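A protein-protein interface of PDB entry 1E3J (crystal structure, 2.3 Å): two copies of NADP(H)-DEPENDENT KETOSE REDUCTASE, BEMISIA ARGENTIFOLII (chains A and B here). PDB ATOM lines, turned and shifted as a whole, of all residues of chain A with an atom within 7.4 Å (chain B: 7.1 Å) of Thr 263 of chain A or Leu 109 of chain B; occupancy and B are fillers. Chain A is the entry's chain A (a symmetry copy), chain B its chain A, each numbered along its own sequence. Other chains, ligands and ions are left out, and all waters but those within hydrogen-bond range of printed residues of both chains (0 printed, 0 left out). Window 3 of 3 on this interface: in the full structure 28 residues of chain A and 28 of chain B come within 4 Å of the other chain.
No position is printed for both chains.
Of the 9 pairs that touch across the chains among the printed residues, none has its exchanged pair printed and touching as well.
The side-chain amide nitrogen (ND2) of Asn 108 of chain B is in hydrogen-bond range of the side-chain carboxylate (OE2) of Glu 288 of chain A (3.2 Å).
A ring nitrogen (NE2) of His 159 of chain B lies within hydrogen-bond range of the side-chain carboxylate (OE2) of Glu 288 of chain A (2.6 Å).
The backbone NH (N) of Phe 295 of chain B sits at hydrogen-bond distance from the side-chain carboxylate (OE2) of Glu 288 of chain A (2.9 Å).
The backbone NH of Gly 264 of chain A lies within hydrogen-bond range of the backbone carbonyl oxygen of Arg 287 of chain A (3.0 Å).
ND2 of Asn 108 of chain B sits at hydrogen-bond distance from O of Phe 295 of chain B (2.9 Å).
The side-chain amide oxygen (OD1) of Asn 108 of chain B is in hydrogen-bond range of the side-chain sulfur (SG) of Cys 298 of chain B (3.4 Å).
The backbone carbonyl oxygen of Phe 101 of chain B is in hydrogen-bond range of the backbone NH of Lys 106 of chain B, at 2.7 Å.
The backbone NH (N) of Phe 101 of chain B sits close to the side-chain sulfur (SG) of Cys 99 of chain B (3.5 Å).
OG1 of Thr 263 of chain A is in hydrogen-bond range of NH1 of Arg 287 of chain A (3.0 Å).
Among the printed residues, pairs that only touch across the chains: Thr 263 of chain A with Phe 101 of chain B, Gly 264 of chain A with Leu 109 of chain B, Thr 263 of chain A with Leu 109 of chain B, Cys 285 of chain A with Phe 295 of chain B, Ala 286 of chain A with Phe 295 of chain B and Glu 288 of chain A with Leu 109 of chain B.
Of the 16 printed residues of chain B, 5 touch a printed residue of chain A.
Hydrophobic or aromatic side chains of chain B that line the printed part of chain A: Phe 101, Leu 109, His 159 and Phe 295.
Among the printed residues, 9 pairs touch across the chains.
Thr 263 of chain A touches just these residues of chain B: Phe 101 (3.4 Å) and Leu 109 (3.7 Å).
Of the printed residues of chain B, Gly 264 of chain A touches Leu 109.
Pro 95 of chain B touches none of the printed residues of chain A.
Of the printed residues of chain A, Phe 101 of chain B touches Thr 263.
Lys 106 of chain B touches none of the printed residues of chain A.
Leu 109 of chain B touches just these residues of chain A: Thr 263, Gly 264 and Glu 288.
The nearest residue of chain B that does not touch Thr 263 of chain A is Cys 110 of chain B (6.2 Å).
The nearest residue of chain A that does not touch Leu 109 of chain B is Arg 287 of chain A (4.2 Å).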
ATOM      1  N   ASP A 239     -19.808   2.075  -5.674  1.00  0.00           N
ATOM      2  CA  ASP A 239     -19.400   2.196  -7.062  1.00  0.00           C
ATOM      3  C   ASP A 239     -18.226   3.153  -7.083  1.00  0.00           C
ATOM      4  O   ASP A 239     -17.874   3.771  -6.076  1.00  0.00           O
ATOM      5  CB  ASP A 239     -20.521   2.801  -7.909  1.00  0.00           C
ATOM      6  CG  ASP A 239     -20.508   2.304  -9.357  1.00  0.00           C
ATOM      7  OD1 ASP A 239     -19.408   2.085  -9.932  1.00  0.00           O
ATOM      8  OD2 ASP A 239     -21.620   2.141  -9.919  1.00  0.00           O
ATOM      9  N   LEU A 240     -17.631   3.270  -8.255  1.00  0.00           N
ATOM     10  CA  LEU A 240     -16.531   4.168  -8.452  1.00  0.00           C
ATOM     11  C   LEU A 240     -17.127   5.568  -8.343  1.00  0.00           C
ATOM     12  O   LEU A 240     -18.332   5.762  -8.602  1.00  0.00           O
ATOM     13  CB  LEU A 240     -15.976   3.945  -9.840  1.00  0.00           C
ATOM     14  CG  LEU A 240     -15.542   2.502  -9.999  1.00  0.00           C
ATOM     15  CD1 LEU A 240     -15.323   2.216 -11.481  1.00  0.00           C
ATOM     16  CD2 LEU A 240     -14.267   2.275  -9.182  1.00  0.00           C
ATOM     17  N   PRO A 241     -16.305   6.549  -7.938  1.00  0.00           N
ATOM     18  CA  PRO A 241     -16.719   7.951  -7.788  1.00  0.00           C
ATOM     19  C   PRO A 241     -17.097   8.479  -9.169  1.00  0.00           C
ATOM     20  O   PRO A 241     -16.383   8.203 -10.108  1.00  0.00           O
ATOM     21  CB  PRO A 241     -15.460   8.630  -7.254  1.00  0.00           C
ATOM     22  CG  PRO A 241     -14.366   7.846  -7.896  1.00  0.00           C
ATOM     23  CD  PRO A 241     -14.851   6.404  -7.776  1.00  0.00           C
ATOM     24  N   ASN A 242     -18.216   9.179  -9.327  1.00  0.00           N
ATOM     25  CA  ASN A 242     -18.484   9.671 -10.665  1.00  0.00           C
ATOM     26  C   ASN A 242     -17.832  11.034 -10.916  1.00  0.00           C
ATOM     27  O   ASN A 242     -17.811  11.526 -12.062  1.00  0.00           O
ATOM     28  CB  ASN A 242     -19.973   9.644 -11.018  1.00  0.00           C
ATOM     29  CG  ASN A 242     -20.840  10.322 -10.009  1.00  0.00           C
ATOM     30  OD1 ASN A 242     -20.670  10.145  -8.806  1.00  0.00           O
ATOM     31  ND2 ASN A 242     -21.827  11.090 -10.500  1.00  0.00           N
ATOM     32  N   ILE A 260      -9.713   5.426 -11.892  1.00  0.00           N
ATOM     33  CA  ILE A 260     -10.668   5.094 -10.852  1.00  0.00           C
ATOM     34  C   ILE A 260     -12.039   5.748 -11.084  1.00  0.00           C
ATOM     35  O   ILE A 260     -13.052   5.329 -10.494  1.00  0.00           O
ATOM     36  CB  ILE A 260     -10.148   5.562  -9.508  1.00  0.00           C
ATOM     37  CG1 ILE A 260     -11.077   5.116  -8.384  1.00  0.00           C
ATOM     38  CG2 ILE A 260     -10.051   7.072  -9.521  1.00  0.00           C
ATOM     39  CD1 ILE A 260     -11.089   3.634  -8.107  1.00  0.00           C
ATOM     40  N   THR A 261     -12.093   6.763 -11.944  1.00  0.00           N
ATOM     41  CA  THR A 261     -13.373   7.443 -12.180  1.00  0.00           C
ATOM     42  C   THR A 261     -14.398   6.580 -12.908  1.00  0.00           C
ATOM     43  O   THR A 261     -14.053   5.863 -13.843  1.00  0.00           O
ATOM     44  CB  THR A 261     -13.181   8.760 -12.965  1.00  0.00           C
ATOM     45  OG1 THR A 261     -12.358   9.655 -12.203  1.00  0.00           O
ATOM     46  CG2 THR A 261     -14.538   9.428 -13.208  1.00  0.00           C
ATOM     47  N   ARG A 262     -15.652   6.640 -12.456  1.00  0.00           N
ATOM     48  CA  ARG A 262     -16.716   5.883 -13.090  1.00  0.00           C
ATOM     49  C   ARG A 262     -16.963   6.287 -14.555  1.00  0.00           C
ATOM     50  O   ARG A 262     -16.856   7.455 -14.923  1.00  0.00           O
ATOM     51  CB  ARG A 262     -18.033   6.065 -12.319  1.00  0.00           C
ATOM     52  CG  ARG A 262     -19.185   5.179 -12.808  1.00  0.00           C
ATOM     53  CD  ARG A 262     -20.547   5.609 -12.181  1.00  0.00           C
ATOM     54  NE  ARG A 262     -20.480   5.670 -10.719  1.00  0.00           N
ATOM     55  CZ  ARG A 262     -21.341   6.327  -9.929  1.00  0.00           C
ATOM     56  NH1 ARG A 262     -22.367   7.015 -10.447  1.00  0.00           N
ATOM     57  NH2 ARG A 262     -21.189   6.272  -8.599  1.00  0.00           N
ATOM     58  N   THR A 263     -17.327   5.314 -15.370  1.00  0.00           N
ATOM     59  CA  THR A 263     -17.638   5.536 -16.770  1.00  0.00           C
ATOM     60  C   THR A 263     -18.652   6.676 -16.850  1.00  0.00           C
ATOM     61  O   THR A 263     -19.605   6.739 -16.067  1.00  0.00           O
ATOM     62  CB  THR A 263     -18.231   4.229 -17.389  1.00  0.00           C
ATOM     63  OG1 THR A 263     -17.234   3.208 -17.344  1.00  0.00           O
ATOM     64  CG2 THR A 263     -18.651   4.415 -18.826  1.00  0.00           C
ATOM     65  N   GLY A 264     -18.422   7.587 -17.776  1.00  0.00           N
ATOM     66  CA  GLY A 264     -19.316   8.722 -17.961  1.00  0.00           C
ATOM     67  C   GLY A 264     -19.154   9.796 -16.913  1.00  0.00           C
ATOM     68  O   GLY A 264     -19.866  10.777 -16.942  1.00  0.00           O
ATOM     69  N   GLY A 265     -18.217   9.602 -15.990  1.00  0.00           N
ATOM     70  CA  GLY A 265     -18.009  10.550 -14.913  1.00  0.00           C
ATOM     71  C   GLY A 265     -17.038  11.618 -15.349  1.00  0.00           C
ATOM     72  O   GLY A 265     -16.719  11.713 -16.546  1.00  0.00           O
ATOM     73  N   THR A 266     -16.542  12.382 -14.382  1.00  0.00           N
ATOM     74  CA  THR A 266     -15.669  13.486 -14.674  1.00  0.00           C
ATOM     75  C   THR A 266     -14.469  13.632 -13.748  1.00  0.00           C
ATOM     76  O   THR A 266     -14.537  13.334 -12.551  1.00  0.00           O
ATOM     77  CB  THR A 266     -16.485  14.805 -14.597  1.00  0.00           C
ATOM     78  OG1 THR A 266     -17.708  14.640 -15.314  1.00  0.00           O
ATOM     79  CG2 THR A 266     -15.708  15.966 -15.178  1.00  0.00           C
ATOM     80  N   ALA A 284      -9.426   7.121 -20.759  1.00  0.00           N
ATOM     81  CA  ALA A 284     -10.523   8.045 -20.501  1.00  0.00           C
ATOM     82  C   ALA A 284     -11.536   7.959 -21.630  1.00  0.00           C
ATOM     83  O   ALA A 284     -12.744   7.869 -21.403  1.00  0.00           O
ATOM     84  CB  ALA A 284      -9.995   9.487 -20.385  1.00  0.00           C
ATOM     85  N   CYS A 285     -11.014   7.977 -22.850  1.00  0.00           N
ATOM     86  CA  CYS A 285     -11.847   7.926 -24.039  1.00  0.00           C
ATOM     87  C   CYS A 285     -12.682   6.639 -24.086  1.00  0.00           C
ATOM     88  O   CYS A 285     -13.891   6.688 -24.323  1.00  0.00           O
ATOM     89  CB  CYS A 285     -10.972   8.067 -25.295  1.00  0.00           C
ATOM     90  SG  CYS A 285     -11.916   8.283 -26.836  1.00  0.00           S
ATOM     91  N   ALA A 286     -12.038   5.506 -23.811  1.00  0.00           N
ATOM     92  CA  ALA A 286     -12.695   4.202 -23.819  1.00  0.00           C
ATOM     93  C   ALA A 286     -13.917   4.122 -22.890  1.00  0.00           C
ATOM     94  O   ALA A 286     -14.726   3.214 -23.034  1.00  0.00           O
ATOM     95  CB  ALA A 286     -11.679   3.101 -23.451  1.00  0.00           C
ATOM     96  N   ARG A 287     -14.062   5.069 -21.956  1.00  0.00           N
ATOM     97  CA  ARG A 287     -15.200   5.074 -21.027  1.00  0.00           C
ATOM     98  C   ARG A 287     -15.850   6.479 -20.896  1.00  0.00           C
ATOM     99  O   ARG A 287     -16.553   6.795 -19.930  1.00  0.00           O
ATOM    100  CB  ARG A 287     -14.719   4.527 -19.672  1.00  0.00           C
ATOM    101  CG  ARG A 287     -14.003   3.150 -19.847  1.00  0.00           C
ATOM    102  CD  ARG A 287     -13.749   2.360 -18.559  1.00  0.00           C
ATOM    103  NE  ARG A 287     -12.810   3.033 -17.659  1.00  0.00           N
ATOM    104  CZ  ARG A 287     -13.193   3.708 -16.574  1.00  0.00           C
ATOM    105  NH1 ARG A 287     -14.490   3.778 -16.274  1.00  0.00           N
ATOM    106  NH2 ARG A 287     -12.301   4.319 -15.804  1.00  0.00           N
ATOM    107  N   GLU A 288     -15.622   7.307 -21.900  1.00  0.00           N
ATOM    108  CA  GLU A 288     -16.131   8.662 -21.923  1.00  0.00           C
ATOM    109  C   GLU A 288     -15.978   9.405 -20.614  1.00  0.00           C
ATOM    110  O   GLU A 288     -16.953   9.958 -20.103  1.00  0.00           O
ATOM    111  CB  GLU A 288     -17.616   8.745 -22.371  1.00  0.00           C
ATOM    112  CG  GLU A 288     -17.820   8.600 -23.861  1.00  0.00           C
ATOM    113  CD  GLU A 288     -19.186   9.112 -24.359  1.00  0.00           C
ATOM    114  OE1 GLU A 288     -20.012   9.571 -23.528  1.00  0.00           O
ATOM    115  OE2 GLU A 288     -19.429   9.055 -25.595  1.00  0.00           O
ATOM    116  N   ILE A 289     -14.779   9.405 -20.051  1.00  0.00           N
ATOM    117  CA  ILE A 289     -14.525  10.183 -18.838  1.00  0.00           C
ATOM    118  C   ILE A 289     -14.212  11.572 -19.415  1.00  0.00           C
ATOM    119  O   ILE A 289     -13.424  11.683 -20.358  1.00  0.00           O
ATOM    120  CB  ILE A 289     -13.221   9.763 -18.118  1.00  0.00           C
ATOM    121  CG1 ILE A 289     -13.257   8.276 -17.721  1.00  0.00           C
ATOM    122  CG2 ILE A 289     -12.967  10.678 -16.910  1.00  0.00           C
ATOM    123  CD1 ILE A 289     -14.211   7.929 -16.624  1.00  0.00           C
ATOM    124  N   ASP A 290     -14.828  12.614 -18.888  1.00  0.00           N
ATOM    125  CA  ASP A 290     -14.514  13.938 -19.333  1.00  0.00           C
ATOM    126  C   ASP A 290     -13.469  14.508 -18.368  1.00  0.00           C
ATOM    127  O   ASP A 290     -13.475  14.192 -17.178  1.00  0.00           O
ATOM    128  CB  ASP A 290     -15.749  14.833 -19.312  1.00  0.00           C
ATOM    129  CG  ASP A 290     -16.801  14.433 -20.373  1.00  0.00           C
ATOM    130  OD1 ASP A 290     -16.472  13.735 -21.369  1.00  0.00           O
ATOM    131  OD2 ASP A 290     -17.974  14.830 -20.206  1.00  0.00           O
ATOM    132  N   PRO B  95     -27.464  -2.407 -26.124  1.00  0.00           N
ATOM    133  CA  PRO B  95     -27.339  -2.313 -24.672  1.00  0.00           C
ATOM    134  C   PRO B  95     -28.277  -3.245 -23.881  1.00  0.00           C
ATOM    135  O   PRO B  95     -29.146  -3.868 -24.473  1.00  0.00           O
ATOM    136  CB  PRO B  95     -27.635  -0.844 -24.420  1.00  0.00           C
ATOM    137  CG  PRO B  95     -28.772  -0.605 -25.343  1.00  0.00           C
ATOM    138  CD  PRO B  95     -28.292  -1.309 -26.644  1.00  0.00           C
ATOM    139  N   CYS B  99     -29.787  -1.059 -17.097  1.00  0.00           N
ATOM    140  CA  CYS B  99     -28.916  -0.538 -16.074  1.00  0.00           C
ATOM    141  C   CYS B  99     -29.164   1.002 -15.955  1.00  0.00           C
ATOM    142  O   CYS B  99     -30.015   1.567 -16.677  1.00  0.00           O
ATOM    143  CB  CYS B  99     -27.461  -0.854 -16.415  1.00  0.00           C
ATOM    144  SG  CYS B  99     -26.928   0.026 -17.841  1.00  0.00           S
ATOM    145  N   PHE B 101     -27.139   3.328 -16.843  1.00  0.00           N
ATOM    146  CA  PHE B 101     -26.655   4.026 -18.050  1.00  0.00           C
ATOM    147  C   PHE B 101     -27.701   3.993 -19.137  1.00  0.00           C
ATOM    148  O   PHE B 101     -27.905   5.003 -19.818  1.00  0.00           O
ATOM    149  CB  PHE B 101     -25.330   3.428 -18.563  1.00  0.00           C
ATOM    150  CG  PHE B 101     -24.175   3.638 -17.621  1.00  0.00           C
ATOM    151  CD1 PHE B 101     -23.556   4.878 -17.531  1.00  0.00           C
ATOM    152  CD2 PHE B 101     -23.706   2.605 -16.837  1.00  0.00           C
ATOM    153  CE1 PHE B 101     -22.478   5.084 -16.661  1.00  0.00           C
ATOM    154  CE2 PHE B 101     -22.636   2.794 -15.965  1.00  0.00           C
ATOM    155  CZ  PHE B 101     -22.020   4.039 -15.883  1.00  0.00           C
ATOM    156  N   CYS B 102     -28.381   2.851 -19.303  1.00  0.00           N
ATOM    157  CA  CYS B 102     -29.431   2.785 -20.335  1.00  0.00           C
ATOM    158  C   CYS B 102     -30.662   3.616 -19.914  1.00  0.00           C
ATOM    159  O   CYS B 102     -31.277   4.291 -20.724  1.00  0.00           O
ATOM    160  CB  CYS B 102     -29.878   1.328 -20.597  1.00  0.00           C
ATOM    161  SG  CYS B 102     -28.529   0.110 -21.115  1.00  0.00           S
ATOM    162  N   LYS B 106     -27.729   6.918 -21.690  1.00  0.00           N
ATOM    163  CA  LYS B 106     -26.308   6.772 -22.067  1.00  0.00           C
ATOM    164  C   LYS B 106     -26.086   5.310 -22.395  1.00  0.00           C
ATOM    165  O   LYS B 106     -25.223   4.673 -21.800  1.00  0.00           O
ATOM    166  CB  LYS B 106     -25.405   7.173 -20.902  1.00  0.00           C
ATOM    167  CG  LYS B 106     -25.582   8.648 -20.501  1.00  0.00           C
ATOM    168  N   TYR B 107     -26.850   4.759 -23.336  1.00  0.00           N
ATOM    169  CA  TYR B 107     -26.670   3.326 -23.564  1.00  0.00           C
ATOM    170  C   TYR B 107     -25.307   2.909 -24.144  1.00  0.00           C
ATOM    171  O   TYR B 107     -24.874   1.784 -23.916  1.00  0.00           O
ATOM    172  CB  TYR B 107     -27.855   2.745 -24.353  1.00  0.00           C
ATOM    173  CG  TYR B 107     -27.956   3.228 -25.767  1.00  0.00           C
ATOM    174  CD1 TYR B 107     -27.044   2.775 -26.753  1.00  0.00           C
ATOM    175  CD2 TYR B 107     -28.948   4.104 -26.138  1.00  0.00           C
ATOM    176  CE1 TYR B 107     -27.153   3.198 -28.088  1.00  0.00           C
ATOM    177  CE2 TYR B 107     -29.058   4.543 -27.455  1.00  0.00           C
ATOM    178  CZ  TYR B 107     -28.156   4.082 -28.429  1.00  0.00           C
ATOM    179  OH  TYR B 107     -28.281   4.520 -29.742  1.00  0.00           O
ATOM    180  N   ASN B 108     -24.594   3.827 -24.814  1.00  0.00           N
ATOM    181  CA  ASN B 108     -23.258   3.491 -25.356  1.00  0.00           C
ATOM    182  C   ASN B 108     -22.299   3.181 -24.220  1.00  0.00           C
ATOM    183  O   ASN B 108     -21.250   2.609 -24.441  1.00  0.00           O
ATOM    184  CB  ASN B 108     -22.693   4.626 -26.217  1.00  0.00           C
ATOM    185  CG  ASN B 108     -22.533   5.916 -25.454  1.00  0.00           C
ATOM    186  OD1 ASN B 108     -23.373   6.274 -24.602  1.00  0.00           O
ATOM    187  ND2 ASN B 108     -21.462   6.644 -25.754  1.00  0.00           N
ATOM    188  N   LEU B 109     -22.660   3.524 -22.987  1.00  0.00           N
ATOM    189  CA  LEU B 109     -21.774   3.220 -21.856  1.00  0.00           C
ATOM    190  C   LEU B 109     -22.288   2.011 -21.060  1.00  0.00           C
ATOM    191  O   LEU B 109     -21.740   1.665 -20.018  1.00  0.00           O
ATOM    192  CB  LEU B 109     -21.711   4.431 -20.924  1.00  0.00           C
ATOM    193  CG  LEU B 109     -21.254   5.738 -21.583  1.00  0.00           C
ATOM    194  CD1 LEU B 109     -21.187   6.838 -20.548  1.00  0.00           C
ATOM    195  CD2 LEU B 109     -19.859   5.507 -22.187  1.00  0.00           C
ATOM    196  N   CYS B 110     -23.346   1.387 -21.533  1.00  0.00           N
ATOM    197  CA  CYS B 110     -23.880   0.235 -20.834  1.00  0.00           C
ATOM    198  C   CYS B 110     -22.765  -0.785 -20.566  1.00  0.00           C
ATOM    199  O   CYS B 110     -21.993  -1.117 -21.463  1.00  0.00           O
ATOM    200  CB  CYS B 110     -24.969  -0.424 -21.691  1.00  0.00           C
ATOM    201  SG  CYS B 110     -25.541  -1.959 -20.987  1.00  0.00           S
ATOM    202  N   PRO B 111     -22.656  -1.292 -19.336  1.00  0.00           N
ATOM    203  CA  PRO B 111     -21.570  -2.265 -19.138  1.00  0.00           C
ATOM    204  C   PRO B 111     -21.789  -3.628 -19.802  1.00  0.00           C
ATOM    205  O   PRO B 111     -20.819  -4.356 -20.013  1.00  0.00           O
ATOM    206  CB  PRO B 111     -21.460  -2.389 -17.607  1.00  0.00           C
ATOM    207  CG  PRO B 111     -22.823  -2.041 -17.143  1.00  0.00           C
ATOM    208  CD  PRO B 111     -23.211  -0.866 -18.047  1.00  0.00           C
ATOM    209  N   ASP B 112     -23.046  -3.978 -20.103  1.00  0.00           N
ATOM    210  CA  ASP B 112     -23.332  -5.259 -20.740  1.00  0.00           C
ATOM    211  C   ASP B 112     -23.674  -5.021 -22.201  1.00  0.00           C
ATOM    212  O   ASP B 112     -24.473  -5.747 -22.802  1.00  0.00           O
ATOM    213  CB  ASP B 112     -24.494  -5.986 -20.060  1.00  0.00           C
ATOM    214  CG  ASP B 112     -24.233  -6.259 -18.578  1.00  0.00           C
ATOM    215  OD1 ASP B 112     -23.063  -6.516 -18.183  1.00  0.00           O
ATOM    216  OD2 ASP B 112     -25.211  -6.222 -17.806  1.00  0.00           O
ATOM    217  N   LEU B 113     -23.085  -3.978 -22.766  1.00  0.00           N
ATOM    218  CA  LEU B 113     -23.326  -3.685 -24.171  1.00  0.00           C
ATOM    219  C   LEU B 113     -22.771  -4.851 -25.028  1.00  0.00           C
ATOM    220  O   LEU B 113     -21.694  -5.395 -24.737  1.00  0.00           O
ATOM    221  CB  LEU B 113     -22.587  -2.397 -24.572  1.00  0.00           C
ATOM    222  CG  LEU B 113     -22.756  -1.835 -25.985  1.00  0.00           C
ATOM    223  CD1 LEU B 113     -24.024  -1.007 -26.119  1.00  0.00           C
ATOM    224  CD2 LEU B 113     -21.586  -0.935 -26.249  1.00  0.00           C
ATOM    225  N   HIS B 159     -21.796  12.170 -33.012  1.00  0.00           N
ATOM    226  CA  HIS B 159     -21.665  12.061 -31.577  1.00  0.00           C
ATOM    227  C   HIS B 159     -20.628  13.046 -31.070  1.00  0.00           C
ATOM    228  O   HIS B 159     -20.863  13.754 -30.077  1.00  0.00           O
ATOM    229  CB  HIS B 159     -21.269  10.649 -31.176  1.00  0.00           C
ATOM    230  CG  HIS B 159     -21.280  10.421 -29.700  1.00  0.00           C
ATOM    231  ND1 HIS B 159     -22.355  10.761 -28.899  1.00  0.00           N
ATOM    232  CD2 HIS B 159     -20.365   9.851 -28.881  1.00  0.00           C
ATOM    233  CE1 HIS B 159     -22.101  10.402 -27.655  1.00  0.00           C
ATOM    234  NE2 HIS B 159     -20.898   9.848 -27.613  1.00  0.00           N
ATOM    235  N   PHE B 295     -17.277   8.124 -27.288  1.00  0.00           N
ATOM    236  CA  PHE B 295     -17.208   6.682 -27.428  1.00  0.00           C
ATOM    237  C   PHE B 295     -18.342   6.192 -28.308  1.00  0.00           C
ATOM    238  O   PHE B 295     -19.486   6.016 -27.841  1.00  0.00           O
ATOM    239  CB  PHE B 295     -17.288   6.005 -26.084  1.00  0.00           C
ATOM    240  CG  PHE B 295     -17.123   4.534 -26.168  1.00  0.00           C
ATOM    241  CD1 PHE B 295     -15.924   3.994 -26.667  1.00  0.00           C
ATOM    242  CD2 PHE B 295     -18.164   3.681 -25.799  1.00  0.00           C
ATOM    243  CE1 PHE B 295     -15.761   2.625 -26.795  1.00  0.00           C
ATOM    244  CE2 PHE B 295     -18.026   2.307 -25.914  1.00  0.00           C
ATOM    245  CZ  PHE B 295     -16.820   1.763 -26.416  1.00  0.00           C
ATOM    246  N   TYR B 297     -21.372   6.129 -30.352  1.00  0.00           N
ATOM    247  CA  TYR B 297     -22.540   6.970 -30.551  1.00  0.00           C
ATOM    248  C   TYR B 297     -23.698   6.559 -29.633  1.00  0.00           C
ATOM    249  O   TYR B 297     -23.741   5.426 -29.103  1.00  0.00           O
ATOM    250  CB  TYR B 297     -22.995   6.878 -32.027  1.00  0.00           C
ATOM    251  CG  TYR B 297     -22.677   5.518 -32.637  1.00  0.00           C
ATOM    252  CD1 TYR B 297     -23.349   4.364 -32.225  1.00  0.00           C
ATOM    253  CD2 TYR B 297     -21.567   5.367 -33.509  1.00  0.00           C
ATOM    254  CE1 TYR B 297     -22.913   3.082 -32.641  1.00  0.00           C
ATOM    255  CE2 TYR B 297     -21.143   4.134 -33.911  1.00  0.00           C
ATOM    256  CZ  TYR B 297     -21.799   2.997 -33.478  1.00  0.00           C
ATOM    257  OH  TYR B 297     -21.279   1.788 -33.816  1.00  0.00           O
ATOM    258  N   CYS B 298     -24.652   7.478 -29.512  1.00  0.00           N
ATOM    259  CA  CYS B 298     -25.813   7.316 -28.646  1.00  0.00           C
ATOM    260  C   CYS B 298     -26.951   8.132 -29.248  1.00  0.00           C
ATOM    261  O   CYS B 298     -26.911   9.375 -29.236  1.00  0.00           O
ATOM    262  CB  CYS B 298     -25.439   7.895 -27.278  1.00  0.00           C
ATOM    263  SG  CYS B 298     -26.349   7.254 -25.901  1.00  0.00           S
